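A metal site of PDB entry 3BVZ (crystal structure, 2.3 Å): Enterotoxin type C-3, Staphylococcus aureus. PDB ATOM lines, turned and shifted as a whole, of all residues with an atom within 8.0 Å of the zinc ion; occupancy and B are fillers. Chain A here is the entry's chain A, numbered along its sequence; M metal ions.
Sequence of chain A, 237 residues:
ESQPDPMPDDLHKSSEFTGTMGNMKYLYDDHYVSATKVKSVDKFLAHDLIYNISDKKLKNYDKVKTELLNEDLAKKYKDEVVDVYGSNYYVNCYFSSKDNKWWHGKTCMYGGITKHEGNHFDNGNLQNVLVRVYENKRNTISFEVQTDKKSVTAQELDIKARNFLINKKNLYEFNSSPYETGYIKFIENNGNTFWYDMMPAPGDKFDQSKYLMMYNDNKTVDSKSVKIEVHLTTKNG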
ATOM      1  N   ALA A  35      21.423   9.764 -24.334  1.00  0.00           N
ATOM      2  CA  ALA A  35      21.817  10.405 -23.100  1.00  0.00           C
ATOM      3  C   ALA A  35      22.234   9.327 -22.151  1.00  0.00           C
ATOM      4  O   ALA A  35      21.679   8.266 -22.132  1.00  0.00           O
ATOM      5  CB  ALA A  35      20.679  11.180 -22.522  1.00  0.00           C
ATOM      6  N   THR A  36      23.207   9.659 -21.326  1.00  0.00           N
ATOM      7  CA  THR A  36      24.015   8.762 -20.543  1.00  0.00           C
ATOM      8  C   THR A  36      23.866   9.130 -19.074  1.00  0.00           C
ATOM      9  O   THR A  36      23.916  10.304 -18.717  1.00  0.00           O
ATOM     10  CB  THR A  36      25.457   8.961 -21.078  1.00  0.00           C
ATOM     11  OG1 THR A  36      25.865   7.784 -21.800  1.00  0.00           O
ATOM     12  CG2 THR A  36      26.432   9.317 -20.008  1.00  0.00           C
ATOM     13  N   LYS A  37      23.616   8.117 -18.228  1.00  0.00           N
ATOM     14  CA  LYS A  37      23.525   8.303 -16.750  1.00  0.00           C
ATOM     15  C   LYS A  37      22.524   9.392 -16.357  1.00  0.00           C
ATOM     16  O   LYS A  37      22.876  10.358 -15.673  1.00  0.00           O
ATOM     17  CB  LYS A  37      24.885   8.589 -16.131  1.00  0.00           C
ATOM     18  CG  LYS A  37      25.870   7.487 -16.300  1.00  0.00           C
ATOM     19  CD  LYS A  37      27.269   7.891 -15.853  1.00  0.00           C
ATOM     20  CE  LYS A  37      27.297   8.091 -14.321  1.00  0.00           C
ATOM     21  NZ  LYS A  37      28.665   8.568 -13.906  1.00  0.00           N
ATOM     22  N   VAL A  38      21.270   9.206 -16.768  1.00  0.00           N
ATOM     23  CA  VAL A  38      20.253  10.196 -16.455  1.00  0.00           C
ATOM     24  C   VAL A  38      19.182   9.638 -15.536  1.00  0.00           C
ATOM     25  O   VAL A  38      18.944   8.444 -15.520  1.00  0.00           O
ATOM     26  CB  VAL A  38      19.650  10.919 -17.731  1.00  0.00           C
ATOM     27  CG1 VAL A  38      20.687  11.846 -18.400  1.00  0.00           C
ATOM     28  CG2 VAL A  38      19.097   9.946 -18.713  1.00  0.00           C
ATOM     29  N   VAL A  81      18.950   5.452 -12.410  1.00  0.00           N
ATOM     30  CA  VAL A  81      19.961   6.053 -13.276  1.00  0.00           C
ATOM     31  C   VAL A  81      20.110   5.139 -14.542  1.00  0.00           C
ATOM     32  O   VAL A  81      20.429   3.952 -14.415  1.00  0.00           O
ATOM     33  CB  VAL A  81      21.312   6.186 -12.543  1.00  0.00           C
ATOM     34  CG1 VAL A  81      22.358   6.820 -13.470  1.00  0.00           C
ATOM     35  CG2 VAL A  81      21.152   7.033 -11.269  1.00  0.00           C
ATOM     36  N   VAL A  82      19.852   5.724 -15.717  1.00  0.00           N
ATOM     37  CA  VAL A  82      19.646   4.960 -16.932  1.00  0.00           C
ATOM     38  C   VAL A  82      20.413   5.569 -18.072  1.00  0.00           C
ATOM     39  O   VAL A  82      20.814   6.729 -18.001  1.00  0.00           O
ATOM     40  CB  VAL A  82      18.093   4.834 -17.343  1.00  0.00           C
ATOM     41  CG1 VAL A  82      17.266   4.155 -16.237  1.00  0.00           C
ATOM     42  CG2 VAL A  82      17.457   6.180 -17.632  1.00  0.00           C
ATOM     43  N   ASP A  83      20.624   4.785 -19.117  1.00  0.00           N
ATOM     44  CA  ASP A  83      21.063   5.317 -20.396  1.00  0.00           C
ATOM     45  C   ASP A  83      19.853   5.274 -21.314  1.00  0.00           C
ATOM     46  O   ASP A  83      18.981   4.450 -21.164  1.00  0.00           O
ATOM     47  CB  ASP A  83      22.252   4.532 -20.974  1.00  0.00           C
ATOM     48  CG  ASP A  83      23.363   4.391 -19.969  1.00  0.00           C
ATOM     49  OD1 ASP A  83      23.629   5.394 -19.278  1.00  0.00           O
ATOM     50  OD2 ASP A  83      23.906   3.277 -19.813  1.00  0.00           O
ATOM     51  N   VAL A  84      19.809   6.211 -22.225  1.00  0.00           N
ATOM     52  CA  VAL A  84      18.722   6.413 -23.099  1.00  0.00           C
ATOM     53  C   VAL A  84      19.262   6.463 -24.548  1.00  0.00           C
ATOM     54  O   VAL A  84      20.264   7.115 -24.827  1.00  0.00           O
ATOM     55  CB  VAL A  84      17.904   7.649 -22.633  1.00  0.00           C
ATOM     56  CG1 VAL A  84      16.763   7.963 -23.588  1.00  0.00           C
ATOM     57  CG2 VAL A  84      17.346   7.355 -21.215  1.00  0.00           C
ATOM     58  N   THR A 114      17.886   1.653 -20.640  1.00  0.00           N
ATOM     59  CA  THR A 114      18.584   0.550 -19.990  1.00  0.00           C
ATOM     60  C   THR A 114      19.194   1.108 -18.711  1.00  0.00           C
ATOM     61  O   THR A 114      19.748   2.192 -18.712  1.00  0.00           O
ATOM     62  CB  THR A 114      19.740  -0.031 -20.899  1.00  0.00           C
ATOM     63  OG1 THR A 114      20.451   1.045 -21.482  1.00  0.00           O
ATOM     64  CG2 THR A 114      19.207  -0.931 -22.085  1.00  0.00           C
ATOM     65  N   LYS A 115      19.091   0.387 -17.600  1.00  0.00           N
ATOM     66  CA  LYS A 115      19.830   0.753 -16.370  1.00  0.00           C
ATOM     67  C   LYS A 115      21.303   0.993 -16.654  1.00  0.00           C
ATOM     68  O   LYS A 115      21.933   0.243 -17.368  1.00  0.00           O
ATOM     69  CB  LYS A 115      19.853  -0.394 -15.377  1.00  0.00           C
ATOM     70  CG  LYS A 115      18.656  -0.608 -14.563  1.00  0.00           C
ATOM     71  CD  LYS A 115      18.767  -2.034 -13.960  1.00  0.00           C
ATOM     72  CE  LYS A 115      17.554  -2.984 -14.364  1.00  0.00           C
ATOM     73  NZ  LYS A 115      17.353  -4.189 -13.394  1.00  0.00           N
ATOM     74  N   HIS A 116      21.874   1.984 -16.035  1.00  0.00           N
ATOM     75  CA  HIS A 116      23.280   2.252 -16.197  1.00  0.00           C
ATOM     76  C   HIS A 116      24.193   1.249 -15.493  1.00  0.00           C
ATOM     77  O   HIS A 116      25.068   0.679 -16.127  1.00  0.00           O
ATOM     78  CB  HIS A 116      23.595   3.646 -15.675  1.00  0.00           C
ATOM     79  CG  HIS A 116      25.053   3.907 -15.513  1.00  0.00           C
ATOM     80  ND1 HIS A 116      25.912   4.026 -16.590  1.00  0.00           N
ATOM     81  CD2 HIS A 116      25.793   4.145 -14.411  1.00  0.00           C
ATOM     82  CE1 HIS A 116      27.117   4.331 -16.156  1.00  0.00           C
ATOM     83  NE2 HIS A 116      27.075   4.412 -14.828  1.00  0.00           N
ATOM     84  N   GLU A 117      23.991   1.094 -14.174  1.00  0.00           N
ATOM     85  CA  GLU A 117      24.899   0.317 -13.320  1.00  0.00           C
ATOM     86  C   GLU A 117      24.926  -1.149 -13.749  1.00  0.00           C
ATOM     87  O   GLU A 117      23.888  -1.787 -13.933  1.00  0.00           O
ATOM     88  CB  GLU A 117      24.521   0.401 -11.799  1.00  0.00           C
ATOM     89  CG  GLU A 117      24.147   1.815 -11.209  1.00  0.00           C
ATOM     90  CD  GLU A 117      25.281   2.904 -11.122  1.00  0.00           C
ATOM     91  OE1 GLU A 117      26.481   2.559 -10.856  1.00  0.00           O
ATOM     92  OE2 GLU A 117      24.917   4.132 -11.276  1.00  0.00           O
ATOM     93  N   GLY A 118      26.126  -1.661 -13.896  1.00  0.00           N
ATOM     94  CA  GLY A 118      26.304  -3.071 -14.170  1.00  0.00           C
ATOM     95  C   GLY A 118      26.219  -3.428 -15.647  1.00  0.00           C
ATOM     96  O   GLY A 118      26.374  -4.596 -16.024  1.00  0.00           O
ATOM     97  N   ASN A 119      25.987  -2.412 -16.498  1.00  0.00           N
ATOM     98  CA  ASN A 119      25.593  -2.702 -17.870  1.00  0.00           C
ATOM     99  C   ASN A 119      26.584  -2.373 -18.958  1.00  0.00           C
ATOM    100  O   ASN A 119      26.154  -2.225 -20.123  1.00  0.00           O
ATOM    101  CB  ASN A 119      24.239  -2.064 -18.245  1.00  0.00           C
ATOM    102  CG  ASN A 119      23.593  -2.784 -19.423  1.00  0.00           C
ATOM    103  OD1 ASN A 119      23.626  -4.019 -19.487  1.00  0.00           O
ATOM    104  ND2 ASN A 119      23.041  -2.036 -20.361  1.00  0.00           N
ATOM    105  N   HIS A 120      27.871  -2.297 -18.594  1.00  0.00           N
ATOM    106  CA  HIS A 120      28.960  -1.988 -19.514  1.00  0.00           C
ATOM    107  C   HIS A 120      30.108  -3.005 -19.445  1.00  0.00           C
ATOM    108  O   HIS A 120      30.315  -3.673 -18.454  1.00  0.00           O
ATOM    109  CB  HIS A 120      29.439  -0.530 -19.369  1.00  0.00           C
ATOM    110  CG  HIS A 120      28.343   0.483 -19.576  1.00  0.00           C
ATOM    111  ND1 HIS A 120      27.693   0.635 -20.778  1.00  0.00           N
ATOM    112  CD2 HIS A 120      27.748   1.349 -18.716  1.00  0.00           C
ATOM    113  CE1 HIS A 120      26.780   1.584 -20.669  1.00  0.00           C
ATOM    114  NE2 HIS A 120      26.787   2.027 -19.426  1.00  0.00           N
ATOM    115  N   ASP A 148      28.458  -0.117 -26.371  1.00  0.00           N
ATOM    116  CA  ASP A 148      29.074  -0.345 -25.064  1.00  0.00           C
ATOM    117  C   ASP A 148      28.165  -1.082 -24.025  1.00  0.00           C
ATOM    118  O   ASP A 148      28.594  -1.355 -22.890  1.00  0.00           O
ATOM    119  CB  ASP A 148      29.552   0.992 -24.474  1.00  0.00           C
ATOM    120  CG  ASP A 148      28.432   1.915 -24.149  1.00  0.00           C
ATOM    121  OD1 ASP A 148      27.320   1.767 -24.695  1.00  0.00           O
ATOM    122  OD2 ASP A 148      28.658   2.830 -23.370  1.00  0.00           O
ATOM    123  N   LYS A 149      26.923  -1.380 -24.390  1.00  0.00           N
ATOM    124  CA  LYS A 149      25.937  -1.935 -23.452  1.00  0.00           C
ATOM    125  C   LYS A 149      25.834  -3.442 -23.526  1.00  0.00           C
ATOM    126  O   LYS A 149      25.760  -4.003 -24.615  1.00  0.00           O
ATOM    127  CB  LYS A 149      24.578  -1.363 -23.743  1.00  0.00           C
ATOM    128  CG  LYS A 149      24.454   0.061 -23.375  1.00  0.00           C
ATOM    129  CD  LYS A 149      23.325   0.691 -24.095  1.00  0.00           C
ATOM    130  CE  LYS A 149      23.193   2.096 -23.606  1.00  0.00           C
ATOM    131  NZ  LYS A 149      22.655   3.029 -24.552  1.00  0.00           N
HETATM  132 ZN    ZN M   1      25.780   3.676 -18.876  1.00  0.00          ZN
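Of the 17 residues printed, 3 come within 4 Å of the zinc ion.
OD1 of Asp 83 sits at hydrogen-bond distance from N of Lys 37 (2.9 Å). O of Thr 114 lies within hydrogen-bond range of N of Asp 83. N of His 116 lies within hydrogen-bond range of O of Val 81, 2.9 Å away. A ring nitrogen (ND1) of His 120 is in hydrogen-bond range of the backbone carbonyl oxygen (O) of Asp 148 (3.0 Å).
NE2 of His 120 is bound to the zinc ion. The zinc ion is bound by OD2 of Asp 83, 2.1 Å away. ND1 of His 116 binds the zinc ion. The zinc ion has three donor atoms within binding distance. Slightly farther from the zinc ion lies OD1 of Asp 83 (2.8 Å).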
